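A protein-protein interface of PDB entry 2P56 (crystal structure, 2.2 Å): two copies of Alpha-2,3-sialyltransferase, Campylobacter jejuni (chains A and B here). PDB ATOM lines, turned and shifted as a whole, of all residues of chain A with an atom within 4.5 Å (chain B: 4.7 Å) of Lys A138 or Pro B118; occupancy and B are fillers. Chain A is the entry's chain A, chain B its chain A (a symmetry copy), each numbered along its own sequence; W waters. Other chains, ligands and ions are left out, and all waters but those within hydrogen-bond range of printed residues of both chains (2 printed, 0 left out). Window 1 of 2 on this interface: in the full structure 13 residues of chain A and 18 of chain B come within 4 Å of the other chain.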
ATOM      1  N   PHE A  99      17.683  -6.999  -5.185  1.00  0.00           N
ATOM      2  CA  PHE A  99      17.249  -7.405  -6.516  1.00  0.00           C
ATOM      3  C   PHE A  99      15.809  -7.923  -6.546  1.00  0.00           C
ATOM      4  O   PHE A  99      15.247  -8.144  -7.618  1.00  0.00           O
ATOM      5  CB  PHE A  99      18.165  -8.505  -7.057  1.00  0.00           C
ATOM      6  CG  PHE A  99      19.609  -8.117  -7.122  1.00  0.00           C
ATOM      7  CD1 PHE A  99      20.469  -8.398  -6.060  1.00  0.00           C
ATOM      8  CD2 PHE A  99      20.108  -7.450  -8.234  1.00  0.00           C
ATOM      9  CE1 PHE A  99      21.804  -8.022  -6.104  1.00  0.00           C
ATOM     10  CE2 PHE A  99      21.447  -7.068  -8.290  1.00  0.00           C
ATOM     11  CZ  PHE A  99      22.298  -7.356  -7.219  1.00  0.00           C
ATOM     12  N   ASN A 100      15.223  -8.104  -5.369  1.00  0.00           N
ATOM     13  CA  ASN A 100      13.871  -8.635  -5.235  1.00  0.00           C
ATOM     14  C   ASN A 100      13.801 -10.023  -5.874  1.00  0.00           C
ATOM     15  O   ASN A 100      13.013 -10.260  -6.790  1.00  0.00           O
ATOM     16  CB  ASN A 100      12.829  -7.709  -5.877  1.00  0.00           C
ATOM     17  CG  ASN A 100      11.389  -8.130  -5.564  1.00  0.00           C
ATOM     18  OD1 ASN A 100      10.430  -7.623  -6.157  1.00  0.00           O
ATOM     19  ND2 ASN A 100      11.233  -9.052  -4.626  1.00  0.00           N
ATOM     20  N   LEU A 101      14.658 -10.923  -5.394  1.00  0.00           N
ATOM     21  CA  LEU A 101      14.698 -12.319  -5.834  1.00  0.00           C
ATOM     22  C   LEU A 101      14.664 -13.113  -4.533  1.00  0.00           C
ATOM     23  O   LEU A 101      15.524 -12.935  -3.660  1.00  0.00           O
ATOM     24  CB  LEU A 101      15.969 -12.613  -6.637  1.00  0.00           C
ATOM     25  CG  LEU A 101      15.873 -12.076  -8.072  1.00  0.00           C
ATOM     26  CD1 LEU A 101      17.217 -12.149  -8.772  1.00  0.00           C
ATOM     27  CD2 LEU A 101      14.803 -12.884  -8.820  1.00  0.00           C
ATOM     28  N   TYR A 134      17.231  -4.289 -15.972  1.00  0.00           N
ATOM     29  CA  TYR A 134      16.693  -5.114 -14.900  1.00  0.00           C
ATOM     30  C   TYR A 134      16.434  -6.545 -15.381  1.00  0.00           C
ATOM     31  O   TYR A 134      16.826  -7.499 -14.720  1.00  0.00           O
ATOM     32  CB  TYR A 134      15.390  -4.505 -14.396  1.00  0.00           C
ATOM     33  CG  TYR A 134      14.941  -4.994 -13.034  1.00  0.00           C
ATOM     34  CD1 TYR A 134      13.654  -5.474 -12.846  1.00  0.00           C
ATOM     35  CD2 TYR A 134      15.774  -4.880 -11.912  1.00  0.00           C
ATOM     36  CE1 TYR A 134      13.187  -5.825 -11.570  1.00  0.00           C
ATOM     37  CE2 TYR A 134      15.319  -5.227 -10.634  1.00  0.00           C
ATOM     38  CZ  TYR A 134      14.024  -5.693 -10.471  1.00  0.00           C
ATOM     39  OH  TYR A 134      13.547  -5.999  -9.214  1.00  0.00           O
ATOM     40  N   ALA A 135      15.768  -6.690 -16.526  1.00  0.00           N
ATOM     41  CA  ALA A 135      15.476  -8.015 -17.068  1.00  0.00           C
ATOM     42  C   ALA A 135      16.783  -8.721 -17.405  1.00  0.00           C
ATOM     43  O   ALA A 135      16.903  -9.950 -17.273  1.00  0.00           O
ATOM     44  CB  ALA A 135      14.600  -7.903 -18.326  1.00  0.00           C
ATOM     45  N   TYR A 136      17.761  -7.937 -17.841  1.00  0.00           N
ATOM     46  CA  TYR A 136      19.066  -8.475 -18.190  1.00  0.00           C
ATOM     47  C   TYR A 136      19.849  -9.027 -16.988  1.00  0.00           C
ATOM     48  O   TYR A 136      20.433 -10.099 -17.079  1.00  0.00           O
ATOM     49  CB  TYR A 136      19.868  -7.400 -18.938  1.00  0.00           C
ATOM     50  CG  TYR A 136      21.372  -7.533 -18.859  1.00  0.00           C
ATOM     51  CD1 TYR A 136      22.090  -6.887 -17.858  1.00  0.00           C
ATOM     52  CD2 TYR A 136      22.080  -8.283 -19.797  1.00  0.00           C
ATOM     53  CE1 TYR A 136      23.481  -6.976 -17.791  1.00  0.00           C
ATOM     54  CE2 TYR A 136      23.478  -8.381 -19.740  1.00  0.00           C
ATOM     55  CZ  TYR A 136      24.168  -7.720 -18.736  1.00  0.00           C
ATOM     56  OH  TYR A 136      25.544  -7.765 -18.686  1.00  0.00           O
ATOM     57  N   ILE A 137      19.861  -8.328 -15.856  1.00  0.00           N
ATOM     58  CA  ILE A 137      20.602  -8.862 -14.713  1.00  0.00           C
ATOM     59  C   ILE A 137      19.874 -10.030 -14.055  1.00  0.00           C
ATOM     60  O   ILE A 137      20.519 -10.948 -13.552  1.00  0.00           O
ATOM     61  CB  ILE A 137      20.949  -7.772 -13.645  1.00  0.00           C
ATOM     62  CG1 ILE A 137      19.686  -7.186 -13.017  1.00  0.00           C
ATOM     63  CG2 ILE A 137      21.777  -6.656 -14.300  1.00  0.00           C
ATOM     64  CD1 ILE A 137      19.987  -6.117 -11.978  1.00  0.00           C
ATOM     65  N   LYS A 138      18.539 -10.023 -14.074  1.00  0.00           N
ATOM     66  CA  LYS A 138      17.795 -11.133 -13.476  1.00  0.00           C
ATOM     67  C   LYS A 138      17.972 -12.402 -14.304  1.00  0.00           C
ATOM     68  O   LYS A 138      18.058 -13.510 -13.761  1.00  0.00           O
ATOM     69  CB  LYS A 138      16.302 -10.788 -13.330  1.00  0.00           C
ATOM     70  CG  LYS A 138      16.061  -9.663 -12.314  1.00  0.00           C
ATOM     71  CD  LYS A 138      14.709  -9.767 -11.636  1.00  0.00           C
ATOM     72  CE  LYS A 138      14.728  -9.029 -10.302  1.00  0.00           C
ATOM     73  NZ  LYS A 138      13.455  -9.200  -9.549  1.00  0.00           N
ATOM     74  N   TYR A 139      18.037 -12.242 -15.622  1.00  0.00           N
ATOM     75  CA  TYR A 139      18.219 -13.387 -16.499  1.00  0.00           C
ATOM     76  C   TYR A 139      19.595 -14.001 -16.206  1.00  0.00           C
ATOM     77  O   TYR A 139      19.723 -15.209 -16.004  1.00  0.00           O
ATOM     78  CB  TYR A 139      18.118 -12.954 -17.967  1.00  0.00           C
ATOM     79  CG  TYR A 139      18.285 -14.089 -18.958  1.00  0.00           C
ATOM     80  CD1 TYR A 139      17.441 -15.199 -18.931  1.00  0.00           C
ATOM     81  CD2 TYR A 139      19.311 -14.064 -19.905  1.00  0.00           C
ATOM     82  CE1 TYR A 139      17.615 -16.257 -19.812  1.00  0.00           C
ATOM     83  CE2 TYR A 139      19.495 -15.119 -20.800  1.00  0.00           C
ATOM     84  CZ  TYR A 139      18.650 -16.209 -20.750  1.00  0.00           C
ATOM     85  OH  TYR A 139      18.839 -17.242 -21.640  1.00  0.00           O
ATOM     86  N   ASN A 140      20.622 -13.163 -16.158  1.00  0.00           N
ATOM     87  CA  ASN A 140      21.967 -13.661 -15.888  1.00  0.00           C
ATOM     88  C   ASN A 140      22.105 -14.269 -14.504  1.00  0.00           C
ATOM     89  O   ASN A 140      22.734 -15.309 -14.344  1.00  0.00           O
ATOM     90  CB  ASN A 140      22.989 -12.546 -16.081  1.00  0.00           C
ATOM     91  CG  ASN A 140      23.279 -12.291 -17.537  1.00  0.00           C
ATOM     92  OD1 ASN A 140      23.907 -13.109 -18.200  1.00  0.00           O
ATOM     93  ND2 ASN A 140      22.809 -11.165 -18.051  1.00  0.00           N
ATOM     94  N   GLU A 141      21.507 -13.624 -13.506  1.00  0.00           N
ATOM     95  CA  GLU A 141      21.555 -14.128 -12.141  1.00  0.00           C
ATOM     96  C   GLU A 141      20.910 -15.501 -12.056  1.00  0.00           C
ATOM     97  O   GLU A 141      21.552 -16.493 -11.711  1.00  0.00           O
ATOM     98  CB  GLU A 141      20.814 -13.169 -11.200  1.00  0.00           C
ATOM     99  CG  GLU A 141      20.602 -13.678  -9.767  1.00  0.00           C
ATOM    100  CD  GLU A 141      21.855 -13.594  -8.895  1.00  0.00           C
ATOM    101  OE1 GLU A 141      22.568 -12.570  -8.963  1.00  0.00           O
ATOM    102  OE2 GLU A 141      22.117 -14.544  -8.124  1.00  0.00           O
ATOM    103  N   ILE A 142      19.628 -15.550 -12.386  1.00  0.00           N
ATOM    104  CA  ILE A 142      18.859 -16.781 -12.311  1.00  0.00           C
ATOM    105  C   ILE A 142      19.348 -17.957 -13.141  1.00  0.00           C
ATOM    106  O   ILE A 142      19.487 -19.075 -12.631  1.00  0.00           O
ATOM    107  CB  ILE A 142      17.381 -16.514 -12.676  1.00  0.00           C
ATOM    108  CG1 ILE A 142      16.773 -15.547 -11.652  1.00  0.00           C
ATOM    109  CG2 ILE A 142      16.594 -17.828 -12.712  1.00  0.00           C
ATOM    110  CD1 ILE A 142      15.443 -14.974 -12.064  1.00  0.00           C
ATOM    111  N   TYR B 114       6.618 -12.155 -11.540  1.00  0.00           N
ATOM    112  CA  TYR B 114       7.387 -11.003 -11.994  1.00  0.00           C
ATOM    113  C   TYR B 114       8.749 -10.881 -11.325  1.00  0.00           C
ATOM    114  O   TYR B 114       9.669 -10.280 -11.893  1.00  0.00           O
ATOM    115  CB  TYR B 114       6.586  -9.704 -11.809  1.00  0.00           C
ATOM    116  CG  TYR B 114       5.394  -9.620 -12.738  1.00  0.00           C
ATOM    117  CD1 TYR B 114       5.557  -9.715 -14.123  1.00  0.00           C
ATOM    118  CD2 TYR B 114       4.096  -9.488 -12.234  1.00  0.00           C
ATOM    119  CE1 TYR B 114       4.450  -9.688 -14.986  1.00  0.00           C
ATOM    120  CE2 TYR B 114       2.993  -9.456 -13.080  1.00  0.00           C
ATOM    121  CZ  TYR B 114       3.175  -9.557 -14.456  1.00  0.00           C
ATOM    122  OH  TYR B 114       2.082  -9.517 -15.293  1.00  0.00           O
ATOM    123  N   ASN B 115       8.905 -11.442 -10.129  1.00  0.00           N
ATOM    124  CA  ASN B 115      10.208 -11.350  -9.474  1.00  0.00           C
ATOM    125  C   ASN B 115      11.239 -12.103 -10.305  1.00  0.00           C
ATOM    126  O   ASN B 115      12.394 -11.702 -10.388  1.00  0.00           O
ATOM    127  CB  ASN B 115      10.160 -11.938  -8.063  1.00  0.00           C
ATOM    128  CG  ASN B 115       9.035 -11.362  -7.234  1.00  0.00           C
ATOM    129  OD1 ASN B 115       7.883 -11.761  -7.369  1.00  0.00           O
ATOM    130  ND2 ASN B 115       9.361 -10.413  -6.384  1.00  0.00           N
ATOM    131  N   PHE B 116      10.804 -13.197 -10.921  1.00  0.00           N
ATOM    132  CA  PHE B 116      11.672 -14.026 -11.749  1.00  0.00           C
ATOM    133  C   PHE B 116      11.694 -13.620 -13.214  1.00  0.00           C
ATOM    134  O   PHE B 116      12.726 -13.735 -13.878  1.00  0.00           O
ATOM    135  CB  PHE B 116      11.232 -15.487 -11.661  1.00  0.00           C
ATOM    136  CG  PHE B 116      11.738 -16.200 -10.445  1.00  0.00           C
ATOM    137  CD1 PHE B 116      13.000 -16.793 -10.448  1.00  0.00           C
ATOM    138  CD2 PHE B 116      10.959 -16.282  -9.296  1.00  0.00           C
ATOM    139  CE1 PHE B 116      13.479 -17.461  -9.326  1.00  0.00           C
ATOM    140  CE2 PHE B 116      11.429 -16.949  -8.163  1.00  0.00           C
ATOM    141  CZ  PHE B 116      12.691 -17.539  -8.179  1.00  0.00           C
ATOM    142  N   PHE B 117      10.555 -13.147 -13.714  1.00  0.00           N
ATOM    143  CA  PHE B 117      10.427 -12.766 -15.123  1.00  0.00           C
ATOM    144  C   PHE B 117       9.830 -11.369 -15.226  1.00  0.00           C
ATOM    145  O   PHE B 117       8.676 -11.199 -15.631  1.00  0.00           O
ATOM    146  CB  PHE B 117       9.527 -13.784 -15.819  1.00  0.00           C
ATOM    147  CG  PHE B 117       9.796 -15.207 -15.402  1.00  0.00           C
ATOM    148  CD1 PHE B 117      10.932 -15.877 -15.849  1.00  0.00           C
ATOM    149  CD2 PHE B 117       8.922 -15.868 -14.548  1.00  0.00           C
ATOM    150  CE1 PHE B 117      11.193 -17.190 -15.454  1.00  0.00           C
ATOM    151  CE2 PHE B 117       9.170 -17.176 -14.145  1.00  0.00           C
ATOM    152  CZ  PHE B 117      10.309 -17.841 -14.598  1.00  0.00           C
ATOM    153  N   PRO B 118      10.622 -10.346 -14.877  1.00  0.00           N
ATOM    154  CA  PRO B 118      10.202  -8.939 -14.901  1.00  0.00           C
ATOM    155  C   PRO B 118       9.632  -8.381 -16.202  1.00  0.00           C
ATOM    156  O   PRO B 118       8.747  -7.536 -16.161  1.00  0.00           O
ATOM    157  CB  PRO B 118      11.458  -8.200 -14.439  1.00  0.00           C
ATOM    158  CG  PRO B 118      12.582  -9.091 -14.909  1.00  0.00           C
ATOM    159  CD  PRO B 118      12.060 -10.465 -14.565  1.00  0.00           C
ATOM    160  N   ASP B 119      10.124  -8.849 -17.348  1.00  0.00           N
ATOM    161  CA  ASP B 119       9.647  -8.358 -18.642  1.00  0.00           C
ATOM    162  C   ASP B 119       8.605  -9.259 -19.290  1.00  0.00           C
ATOM    163  O   ASP B 119       8.226  -9.033 -20.438  1.00  0.00           O
ATOM    164  CB  ASP B 119      10.828  -8.167 -19.609  1.00  0.00           C
ATOM    165  CG  ASP B 119      11.612  -9.445 -19.832  1.00  0.00           C
ATOM    166  OD1 ASP B 119      11.315 -10.452 -19.151  1.00  0.00           O
ATOM    167  OD2 ASP B 119      12.525  -9.445 -20.683  1.00  0.00           O
ATOM    168  N   ALA B 120       8.152 -10.280 -18.559  1.00  0.00           N
ATOM    169  CA  ALA B 120       7.143 -11.195 -19.071  1.00  0.00           C
ATOM    170  C   ALA B 120       5.757 -10.685 -18.657  1.00  0.00           C
ATOM    171  O   ALA B 120       5.648  -9.667 -17.978  1.00  0.00           O
ATOM    172  CB  ALA B 120       7.385 -12.602 -18.526  1.00  0.00           C
HETATM  173  O   HOH W   1      15.136 -14.111 -15.702  1.00  0.00           O
HETATM  174  O   HOH W   2      11.306  -8.246 -10.766  1.00  0.00           O
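The side-chain amide nitrogen (ND2) of Asn A100 sits close to the side-chain amide nitrogen (ND2) of Asn B115, at 2.9 Å.
The side-chain amino group of Lys A138 sits at hydrogen-bond distance from the backbone carbonyl oxygen of Asn B115, at 2.8 Å.
NZ of Lys A138 lies within hydrogen-bond range of OH of Tyr A134, at 3.2 Å.
The backbone carbonyl oxygen of Phe A99 is in hydrogen-bond range of the side-chain hydroxyl of Tyr A134.
The backbone carbonyl oxygen (O) of Asn A100 lies within hydrogen-bond range of the side-chain amino group (NZ) of Lys A138 (3.0 Å).
O of Phe A99 is in hydrogen-bond range of NZ of Lys A138 (2.8 Å).
Among the printed residues, merely in contact across the chains: Leu A101 with Asn B115 (3.1 Å), Tyr A134 with Pro B118 (3.8 Å), Ala A135 with Pro B118 (3.8 Å), Ala A135 with Asp B119 (3.5 Å), Lys A138 with Pro B118 (3.96 Å) and Ile A142 with Phe B116 (3.4 Å).
Printed residues of chain B within 4 Å of Tyr A134: Pro B118.
Lys A138 touches two residues of chain B.
Glu A141 touches none of the printed residues of chain B.
Of the printed residues of chain B, Ile A142 touches Phe B116.
Printed residues of chain A within 4 Å of Phe B116: Ile A142 (3.4 Å).
Pro B118 touches just these residues of chain A: Tyr A134, Ala A135 and Lys A138.
Of the printed residues of chain A, Asp B119 touches Ala A135.
The nearest residue of chain B that does not touch Lys A138 is Tyr B114 (4.6 Å).
Among the printed residues, 8 pairs touch across the chains.
Among the printed residues, no Asp or Glu carboxylate lies within 4 Å of a Lys or Arg side-chain nitrogen of the other chain.
No position is printed for both chains.
Water W2 lies within hydrogen-bond range of NZ of Lys A138 (2.6 Å) and O of Tyr B114 (2.8 Å).
Water W1 bridges O of Phe B116 (3.0 Å) and N of Tyr A139 (3.5 Å).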
